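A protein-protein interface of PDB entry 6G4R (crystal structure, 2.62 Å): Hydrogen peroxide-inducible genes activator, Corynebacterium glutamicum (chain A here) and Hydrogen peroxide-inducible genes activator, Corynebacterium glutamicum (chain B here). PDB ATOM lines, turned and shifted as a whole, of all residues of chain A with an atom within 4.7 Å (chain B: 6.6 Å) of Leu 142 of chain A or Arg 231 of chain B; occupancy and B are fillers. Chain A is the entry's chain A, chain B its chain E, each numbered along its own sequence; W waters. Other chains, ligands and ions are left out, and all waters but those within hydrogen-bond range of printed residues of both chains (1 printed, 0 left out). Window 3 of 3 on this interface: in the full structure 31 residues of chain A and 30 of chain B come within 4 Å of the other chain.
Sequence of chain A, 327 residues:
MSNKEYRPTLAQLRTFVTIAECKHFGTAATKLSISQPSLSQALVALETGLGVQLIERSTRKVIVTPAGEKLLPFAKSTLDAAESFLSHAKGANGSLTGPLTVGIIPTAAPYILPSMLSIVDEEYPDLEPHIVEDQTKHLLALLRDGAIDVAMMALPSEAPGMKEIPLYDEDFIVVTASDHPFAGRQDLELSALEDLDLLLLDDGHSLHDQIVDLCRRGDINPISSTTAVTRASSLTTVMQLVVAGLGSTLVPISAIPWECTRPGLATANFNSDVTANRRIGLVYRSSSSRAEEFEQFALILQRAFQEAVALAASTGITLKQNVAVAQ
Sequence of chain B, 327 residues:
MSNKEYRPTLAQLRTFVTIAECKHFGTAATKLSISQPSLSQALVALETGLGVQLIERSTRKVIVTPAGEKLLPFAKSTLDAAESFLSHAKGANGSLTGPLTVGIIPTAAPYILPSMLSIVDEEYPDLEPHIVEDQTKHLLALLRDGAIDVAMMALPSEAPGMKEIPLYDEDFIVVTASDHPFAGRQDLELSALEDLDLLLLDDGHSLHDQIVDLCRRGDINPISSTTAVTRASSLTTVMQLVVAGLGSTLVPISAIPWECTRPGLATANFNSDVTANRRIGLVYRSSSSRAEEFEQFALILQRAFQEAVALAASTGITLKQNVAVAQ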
ATOM      1  N   ILE A 131      14.450 -15.972 -32.322  1.00  0.00           N
ATOM      2  CA  ILE A 131      15.005 -15.279 -31.167  1.00  0.00           C
ATOM      3  C   ILE A 131      13.867 -14.796 -30.283  1.00  0.00           C
ATOM      4  O   ILE A 131      12.870 -14.253 -30.775  1.00  0.00           O
ATOM      5  CB  ILE A 131      15.896 -14.104 -31.613  1.00  0.00           C
ATOM      6  CG1 ILE A 131      16.863 -14.552 -32.710  1.00  0.00           C
ATOM      7  CG2 ILE A 131      16.655 -13.530 -30.427  1.00  0.00           C
ATOM      8  CD1 ILE A 131      17.797 -15.661 -32.289  1.00  0.00           C
ATOM      9  N   VAL A 132      14.005 -14.990 -28.974  1.00  0.00           N
ATOM     10  CA  VAL A 132      13.045 -14.460 -28.008  1.00  0.00           C
ATOM     11  C   VAL A 132      13.830 -13.593 -27.033  1.00  0.00           C
ATOM     12  O   VAL A 132      14.649 -14.106 -26.262  1.00  0.00           O
ATOM     13  CB  VAL A 132      12.286 -15.562 -27.254  1.00  0.00           C
ATOM     14  CG1 VAL A 132      11.459 -14.956 -26.129  1.00  0.00           C
ATOM     15  CG2 VAL A 132      11.389 -16.351 -28.199  1.00  0.00           C
ATOM     16  N   GLU A 133      13.591 -12.284 -27.066  1.00  0.00           N
ATOM     17  CA  GLU A 133      14.274 -11.343 -26.187  1.00  0.00           C
ATOM     18  C   GLU A 133      13.328 -10.911 -25.073  1.00  0.00           C
ATOM     19  O   GLU A 133      12.309 -10.262 -25.335  1.00  0.00           O
ATOM     20  CB  GLU A 133      14.770 -10.123 -26.963  1.00  0.00           C
ATOM     21  CG  GLU A 133      15.528  -9.123 -26.103  1.00  0.00           C
ATOM     22  CD  GLU A 133      15.667  -7.766 -26.763  1.00  0.00           C
ATOM     23  OE1 GLU A 133      14.737  -7.356 -27.487  1.00  0.00           O
ATOM     24  OE2 GLU A 133      16.708  -7.107 -26.555  1.00  0.00           O
ATOM     25  N   HIS A 138      11.296 -14.106 -17.031  1.00  0.00           N
ATOM     26  CA  HIS A 138      10.329 -14.545 -18.032  1.00  0.00           C
ATOM     27  C   HIS A 138      10.927 -15.605 -18.951  1.00  0.00           C
ATOM     28  O   HIS A 138      10.198 -16.465 -19.458  1.00  0.00           O
ATOM     29  CB  HIS A 138       9.829 -13.352 -18.852  1.00  0.00           C
ATOM     30  CG  HIS A 138       8.765 -13.703 -19.848  1.00  0.00           C
ATOM     31  ND1 HIS A 138       8.911 -13.485 -21.201  1.00  0.00           N
ATOM     32  CD2 HIS A 138       7.541 -14.259 -19.688  1.00  0.00           C
ATOM     33  CE1 HIS A 138       7.822 -13.889 -21.831  1.00  0.00           C
ATOM     34  NE2 HIS A 138       6.975 -14.363 -20.936  1.00  0.00           N
ATOM     35  N   LEU A 139      12.242 -15.555 -19.183  1.00  0.00           N
ATOM     36  CA  LEU A 139      12.898 -16.576 -19.996  1.00  0.00           C
ATOM     37  C   LEU A 139      12.841 -17.939 -19.317  1.00  0.00           C
ATOM     38  O   LEU A 139      12.522 -18.949 -19.956  1.00  0.00           O
ATOM     39  CB  LEU A 139      14.348 -16.179 -20.278  1.00  0.00           C
ATOM     40  CG  LEU A 139      14.597 -15.038 -21.267  1.00  0.00           C
ATOM     41  CD1 LEU A 139      16.081 -14.921 -21.577  1.00  0.00           C
ATOM     42  CD2 LEU A 139      13.797 -15.241 -22.545  1.00  0.00           C
ATOM     43  N   LEU A 140      13.161 -17.988 -18.021  1.00  0.00           N
ATOM     44  CA  LEU A 140      13.086 -19.248 -17.289  1.00  0.00           C
ATOM     45  C   LEU A 140      11.662 -19.780 -17.238  1.00  0.00           C
ATOM     46  O   LEU A 140      11.455 -20.999 -17.236  1.00  0.00           O
ATOM     47  CB  LEU A 140      13.640 -19.073 -15.874  1.00  0.00           C
ATOM     48  CG  LEU A 140      15.150 -18.856 -15.769  1.00  0.00           C
ATOM     49  CD1 LEU A 140      15.549 -18.504 -14.343  1.00  0.00           C
ATOM     50  CD2 LEU A 140      15.894 -20.093 -16.248  1.00  0.00           C
ATOM     51  N   ALA A 141      10.671 -18.888 -17.181  1.00  0.00           N
ATOM     52  CA  ALA A 141       9.283 -19.328 -17.257  1.00  0.00           C
ATOM     53  C   ALA A 141       9.000 -19.994 -18.598  1.00  0.00           C
ATOM     54  O   ALA A 141       8.479 -21.114 -18.650  1.00  0.00           O
ATOM     55  CB  ALA A 141       8.344 -18.143 -17.028  1.00  0.00           C
ATOM     56  N   LEU A 142       9.373 -19.333 -19.698  1.00  0.00           N
ATOM     57  CA  LEU A 142       9.186 -19.922 -21.021  1.00  0.00           C
ATOM     58  C   LEU A 142      10.014 -21.185 -21.216  1.00  0.00           C
ATOM     59  O   LEU A 142       9.679 -22.003 -22.079  1.00  0.00           O
ATOM     60  CB  LEU A 142       9.535 -18.905 -22.109  1.00  0.00           C
ATOM     61  CG  LEU A 142       8.665 -17.651 -22.201  1.00  0.00           C
ATOM     62  CD1 LEU A 142       9.194 -16.722 -23.283  1.00  0.00           C
ATOM     63  CD2 LEU A 142       7.216 -18.017 -22.469  1.00  0.00           C
ATOM     64  N   LEU A 143      11.083 -21.362 -20.439  1.00  0.00           N
ATOM     65  CA  LEU A 143      11.902 -22.559 -20.573  1.00  0.00           C
ATOM     66  C   LEU A 143      11.255 -23.753 -19.882  1.00  0.00           C
ATOM     67  O   LEU A 143      11.306 -24.876 -20.398  1.00  0.00           O
ATOM     68  CB  LEU A 143      13.300 -22.305 -20.006  1.00  0.00           C
ATOM     69  CG  LEU A 143      14.379 -23.333 -20.354  1.00  0.00           C
ATOM     70  CD1 LEU A 143      14.498 -23.497 -21.862  1.00  0.00           C
ATOM     71  CD2 LEU A 143      15.715 -22.935 -19.747  1.00  0.00           C
ATOM     72  N   ARG A 144      10.645 -23.532 -18.714  1.00  0.00           N
ATOM     73  CA  ARG A 144       9.920 -24.603 -18.039  1.00  0.00           C
ATOM     74  C   ARG A 144       8.696 -25.038 -18.835  1.00  0.00           C
ATOM     75  O   ARG A 144       8.435 -26.239 -18.977  1.00  0.00           O
ATOM     76  CB  ARG A 144       9.513 -24.159 -16.634  1.00  0.00           C
ATOM     77  CG  ARG A 144      10.606 -24.321 -15.594  1.00  0.00           C
ATOM     78  CD  ARG A 144      10.099 -23.994 -14.202  1.00  0.00           C
ATOM     79  NE  ARG A 144       9.710 -22.593 -14.077  1.00  0.00           N
ATOM     80  CZ  ARG A 144      10.538 -21.620 -13.709  1.00  0.00           C
ATOM     81  NH1 ARG A 144      11.804 -21.896 -13.426  1.00  0.00           N
ATOM     82  NH2 ARG A 144      10.101 -20.371 -13.620  1.00  0.00           N
ATOM     83  N   ASP A 145       7.933 -24.081 -19.361  1.00  0.00           N
ATOM     84  CA  ASP A 145       6.719 -24.385 -20.109  1.00  0.00           C
ATOM     85  C   ASP A 145       6.996 -24.840 -21.538  1.00  0.00           C
ATOM     86  O   ASP A 145       6.050 -24.980 -22.320  1.00  0.00           O
ATOM     87  CB  ASP A 145       5.790 -23.167 -20.125  1.00  0.00           C
ATOM     88  CG  ASP A 145       5.370 -22.734 -18.733  1.00  0.00           C
ATOM     89  OD1 ASP A 145       5.859 -21.690 -18.256  1.00  0.00           O
ATOM     90  OD2 ASP A 145       4.556 -23.443 -18.108  1.00  0.00           O
ATOM     91  N   GLY A 146       8.257 -25.073 -21.896  1.00  0.00           N
ATOM     92  CA  GLY A 146       8.583 -25.565 -23.220  1.00  0.00           C
ATOM     93  C   GLY A 146       8.451 -24.565 -24.344  1.00  0.00           C
ATOM     94  O   GLY A 146       8.595 -24.948 -25.509  1.00  0.00           O
ATOM     95  N   ALA A 147       8.172 -23.294 -24.039  1.00  0.00           N
ATOM     96  CA  ALA A 147       7.971 -22.305 -25.091  1.00  0.00           C
ATOM     97  C   ALA A 147       9.265 -21.960 -25.816  1.00  0.00           C
ATOM     98  O   ALA A 147       9.216 -21.535 -26.976  1.00  0.00           O
ATOM     99  CB  ALA A 147       7.344 -21.038 -24.511  1.00  0.00           C
ATOM    100  N   ILE A 148      10.413 -22.132 -25.165  1.00  0.00           N
ATOM    101  CA  ILE A 148      11.715 -21.956 -25.795  1.00  0.00           C
ATOM    102  C   ILE A 148      12.564 -23.182 -25.488  1.00  0.00           C
ATOM    103  O   ILE A 148      12.351 -23.875 -24.487  1.00  0.00           O
ATOM    104  CB  ILE A 148      12.430 -20.665 -25.329  1.00  0.00           C
ATOM    105  CG1 ILE A 148      12.849 -20.776 -23.862  1.00  0.00           C
ATOM    106  CG2 ILE A 148      11.547 -19.445 -25.550  1.00  0.00           C
ATOM    107  CD1 ILE A 148      13.572 -19.552 -23.341  1.00  0.00           C
ATOM    108  N   LEU B 199       8.213  -7.776 -38.019  1.00  0.00           N
ATOM    109  CA  LEU B 199       8.793  -8.094 -36.718  1.00  0.00           C
ATOM    110  C   LEU B 199       8.329  -7.047 -35.713  1.00  0.00           C
ATOM    111  O   LEU B 199       8.672  -5.865 -35.829  1.00  0.00           O
ATOM    112  CB  LEU B 199      10.316  -8.148 -36.793  1.00  0.00           C
ATOM    113  CG  LEU B 199      10.896  -9.253 -37.678  1.00  0.00           C
ATOM    114  CD1 LEU B 199      12.377  -9.018 -37.935  1.00  0.00           C
ATOM    115  CD2 LEU B 199      10.668 -10.617 -37.041  1.00  0.00           C
ATOM    116  N   LEU B 200       7.545  -7.488 -34.737  1.00  0.00           N
ATOM    117  CA  LEU B 200       6.870  -6.623 -33.785  1.00  0.00           C
ATOM    118  C   LEU B 200       7.462  -6.786 -32.392  1.00  0.00           C
ATOM    119  O   LEU B 200       8.020  -7.831 -32.047  1.00  0.00           O
ATOM    120  CB  LEU B 200       5.364  -6.905 -33.729  1.00  0.00           C
ATOM    121  CG  LEU B 200       4.532  -6.864 -35.015  1.00  0.00           C
ATOM    122  CD1 LEU B 200       4.947  -5.692 -35.895  1.00  0.00           C
ATOM    123  CD2 LEU B 200       4.589  -8.184 -35.780  1.00  0.00           C
ATOM    124  N   LEU B 201       7.334  -5.728 -31.600  1.00  0.00           N
ATOM    125  CA  LEU B 201       7.650  -5.806 -30.187  1.00  0.00           C
ATOM    126  C   LEU B 201       6.544  -6.583 -29.477  1.00  0.00           C
ATOM    127  O   LEU B 201       5.432  -6.729 -29.992  1.00  0.00           O
ATOM    128  CB  LEU B 201       7.796  -4.403 -29.595  1.00  0.00           C
ATOM    129  CG  LEU B 201       9.017  -3.598 -30.051  1.00  0.00           C
ATOM    130  CD1 LEU B 201       8.809  -2.112 -29.793  1.00  0.00           C
ATOM    131  CD2 LEU B 201      10.284  -4.085 -29.370  1.00  0.00           C
ATOM    132  N   ASP B 202       6.868  -7.118 -28.303  1.00  0.00           N
ATOM    133  CA  ASP B 202       5.958  -8.021 -27.603  1.00  0.00           C
ATOM    134  C   ASP B 202       4.700  -7.276 -27.146  1.00  0.00           C
ATOM    135  O   ASP B 202       4.448  -6.126 -27.511  1.00  0.00           O
ATOM    136  CB  ASP B 202       6.666  -8.698 -26.430  1.00  0.00           C
ATOM    137  CG  ASP B 202       7.202  -7.708 -25.404  1.00  0.00           C
ATOM    138  OD1 ASP B 202       7.065  -6.483 -25.607  1.00  0.00           O
ATOM    139  OD2 ASP B 202       7.751  -8.162 -24.376  1.00  0.00           O
ATOM    140  N   ASP B 203       3.904  -7.933 -26.303  1.00  0.00           N
ATOM    141  CA  ASP B 203       2.539  -7.483 -26.065  1.00  0.00           C
ATOM    142  C   ASP B 203       2.436  -6.284 -25.132  1.00  0.00           C
ATOM    143  O   ASP B 203       1.410  -5.597 -25.153  1.00  0.00           O
ATOM    144  CB  ASP B 203       1.705  -8.639 -25.513  1.00  0.00           C
ATOM    145  CG  ASP B 203       1.407  -9.689 -26.563  1.00  0.00           C
ATOM    146  OD1 ASP B 203       2.342 -10.424 -26.949  1.00  0.00           O
ATOM    147  OD2 ASP B 203       0.244  -9.778 -27.007  1.00  0.00           O
ATOM    148  N   ALA B 228       5.350 -14.556 -35.659  1.00  0.00           N
ATOM    149  CA  ALA B 228       4.504 -14.981 -34.549  1.00  0.00           C
ATOM    150  C   ALA B 228       5.347 -15.501 -33.390  1.00  0.00           C
ATOM    151  O   ALA B 228       5.079 -15.194 -32.229  1.00  0.00           O
ATOM    152  CB  ALA B 228       3.521 -16.047 -35.010  1.00  0.00           C
ATOM    153  N   VAL B 229       6.370 -16.289 -33.712  1.00  0.00           N
ATOM    154  CA  VAL B 229       7.244 -16.850 -32.687  1.00  0.00           C
ATOM    155  C   VAL B 229       8.388 -15.900 -32.352  1.00  0.00           C
ATOM    156  O   VAL B 229       8.725 -15.719 -31.179  1.00  0.00           O
ATOM    157  CB  VAL B 229       7.758 -18.235 -33.138  1.00  0.00           C
ATOM    158  CG1 VAL B 229       8.263 -18.181 -34.572  1.00  0.00           C
ATOM    159  CG2 VAL B 229       8.841 -18.741 -32.196  1.00  0.00           C
ATOM    160  N   THR B 230       9.001 -15.284 -33.365  1.00  0.00           N
ATOM    161  CA  THR B 230      10.066 -14.319 -33.123  1.00  0.00           C
ATOM    162  C   THR B 230       9.513 -13.134 -32.345  1.00  0.00           C
ATOM    163  O   THR B 230       8.461 -12.588 -32.688  1.00  0.00           O
ATOM    164  CB  THR B 230      10.672 -13.852 -34.446  1.00  0.00           C
ATOM    165  OG1 THR B 230      11.194 -14.979 -35.160  1.00  0.00           O
ATOM    166  CG2 THR B 230      11.795 -12.853 -34.198  1.00  0.00           C
ATOM    167  N   ARG B 231      10.221 -12.733 -31.291  1.00  0.00           N
ATOM    168  CA  ARG B 231       9.688 -11.716 -30.391  1.00  0.00           C
ATOM    169  C   ARG B 231      10.830 -11.034 -29.653  1.00  0.00           C
ATOM    170  O   ARG B 231      11.620 -11.697 -28.974  1.00  0.00           O
ATOM    171  CB  ARG B 231       8.681 -12.372 -29.440  1.00  0.00           C
ATOM    172  CG  ARG B 231       7.876 -11.460 -28.547  1.00  0.00           C
ATOM    173  CD  ARG B 231       6.596 -12.177 -28.111  1.00  0.00           C
ATOM    174  NE  ARG B 231       6.790 -13.577 -27.736  1.00  0.00           N
ATOM    175  CZ  ARG B 231       7.185 -14.003 -26.542  1.00  0.00           C
ATOM    176  NH1 ARG B 231       7.437 -13.137 -25.571  1.00  0.00           N
ATOM    177  NH2 ARG B 231       7.322 -15.305 -26.319  1.00  0.00           N
ATOM    178  N   ALA B 232      10.913  -9.712 -29.795  1.00  0.00           N
ATOM    179  CA  ALA B 232      11.940  -8.890 -29.176  1.00  0.00           C
ATOM    180  C   ALA B 232      11.308  -7.849 -28.260  1.00  0.00           C
ATOM    181  O   ALA B 232      10.119  -7.536 -28.367  1.00  0.00           O
ATOM    182  CB  ALA B 232      12.808  -8.195 -30.235  1.00  0.00           C
ATOM    183  N   SER B 233      12.123  -7.313 -27.352  1.00  0.00           N
ATOM    184  CA  SER B 233      11.668  -6.313 -26.397  1.00  0.00           C
ATOM    185  C   SER B 233      12.199  -4.913 -26.675  1.00  0.00           C
ATOM    186  O   SER B 233      11.747  -3.962 -26.028  1.00  0.00           O
ATOM    187  CB  SER B 233      12.062  -6.723 -24.970  1.00  0.00           C
ATOM    188  OG  SER B 233      13.456  -6.585 -24.766  1.00  0.00           O
ATOM    189  N   THR B 237      17.201  -4.525 -30.988  1.00  0.00           N
ATOM    190  CA  THR B 237      17.254  -5.952 -31.284  1.00  0.00           C
ATOM    191  C   THR B 237      16.488  -6.274 -32.562  1.00  0.00           C
ATOM    192  O   THR B 237      16.932  -7.101 -33.367  1.00  0.00           O
ATOM    193  CB  THR B 237      16.700  -6.754 -30.106  1.00  0.00           C
ATOM    194  OG1 THR B 237      17.468  -6.468 -28.930  1.00  0.00           O
ATOM    195  CG2 THR B 237      16.762  -8.247 -30.392  1.00  0.00           C
ATOM    196  N   VAL B 238      15.335  -5.630 -32.762  1.00  0.00           N
ATOM    197  CA  VAL B 238      14.578  -5.812 -33.997  1.00  0.00           C
ATOM    198  C   VAL B 238      15.415  -5.403 -35.202  1.00  0.00           C
ATOM    199  O   VAL B 238      15.379  -6.054 -36.253  1.00  0.00           O
ATOM    200  CB  VAL B 238      13.253  -5.028 -33.930  1.00  0.00           C
ATOM    201  CG1 VAL B 238      12.556  -5.029 -35.281  1.00  0.00           C
ATOM    202  CG2 VAL B 238      12.346  -5.614 -32.860  1.00  0.00           C
ATOM    203  N   LEU B 241      17.718  -8.047 -36.395  1.00  0.00           N
ATOM    204  CA  LEU B 241      16.999  -9.094 -37.113  1.00  0.00           C
ATOM    205  C   LEU B 241      16.677  -8.662 -38.537  1.00  0.00           C
ATOM    206  O   LEU B 241      16.682  -9.487 -39.459  1.00  0.00           O
ATOM    207  CB  LEU B 241      15.719  -9.462 -36.364  1.00  0.00           C
ATOM    208  CG  LEU B 241      15.889  -9.902 -34.909  1.00  0.00           C
ATOM    209  CD1 LEU B 241      14.545 -10.245 -34.291  1.00  0.00           C
ATOM    210  CD2 LEU B 241      16.840 -11.077 -34.817  1.00  0.00           C
HETATM  211  O   HOH W   1      17.981  -4.724 -26.007  1.00  0.00           O
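OG1 of Thr 237 of chain B lies within hydrogen-bond range of OE2 of Glu 133 of chain A, 2.6 Å away. The backbone NH (N) of Glu 133 of chain A sits at hydrogen-bond distance from the backbone carbonyl oxygen (O) of Arg 231 of chain B (2.8 Å). The backbone NH of Ser 233 of chain B lies within hydrogen-bond range of the side-chain carboxylate of Glu 133 of chain A, at 2.6 Å. O of Ile 131 of chain A sits at hydrogen-bond distance from N of Arg 231 of chain B, at 3.1 Å.
N of Asp 202 of chain B is in hydrogen-bond range of O of Ala 232 of chain B (3.3 Å). N of Ile 148 of chain A is in hydrogen-bond range of O of Leu 142 of chain A, at 3.2 Å. N of Ala 147 of chain A sits at hydrogen-bond distance from O of Leu 142 of chain A (2.8 Å).
Thr 230 of chain B touches Ile 131 of chain A (CA to O, 3.7 Å). CA of Val 132 of chain A touches O of Arg 231 of chain B (3.3 Å). OE1 of Glu 133 of chain A touches CB of Ala 232 of chain B, at 3.5 Å. Arg 231 of chain B touches His 138 of chain A. Leu 142 of chain A touches Arg 231 of chain B.
Leu 142 of chain A touches just one residue of chain B: Arg 231. Printed residues of chain A within 4 Å of Arg 231 of chain B: Ile 131, Val 132, Glu 133, His 138 and Leu 142. Printed residues of chain B within 4 Å of His 138 of chain A: Arg 231. Printed residues of chain A within 4 Å of Ser 233 of chain B: Glu 133. Asp 145 of chain A touches none of the printed residues of chain B. Ile 148 of chain A touches none of the printed residues of chain B. The nearest printed residue of chain B that does not touch Leu 142 of chain A is Val 229 of chain B (8.0 Å). The nearest printed residue of chain B that does not touch His 138 of chain A is Asp 202 of chain B (6.3 Å).
Hydrophobic or aromatic side chains of chain B within 4 Å of the printed part of chain A: Ala 232. Of the 14 printed residues of chain A, 5 touch a printed residue of chain B. Along chain A the printed residues that touch a printed residue of chain B span positions 131 to 142. Among the printed residues, 9 pairs touch across the chains. Among the printed residues, no Asp or Glu carboxylate lies within 4 Å of a Lys or Arg side-chain nitrogen of the other chain.
Water W1 lies within hydrogen-bond range of OE2 of Glu 133 of chain A (2.8 Å) and OG1 of Thr 237 of chain B (3.4 Å).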
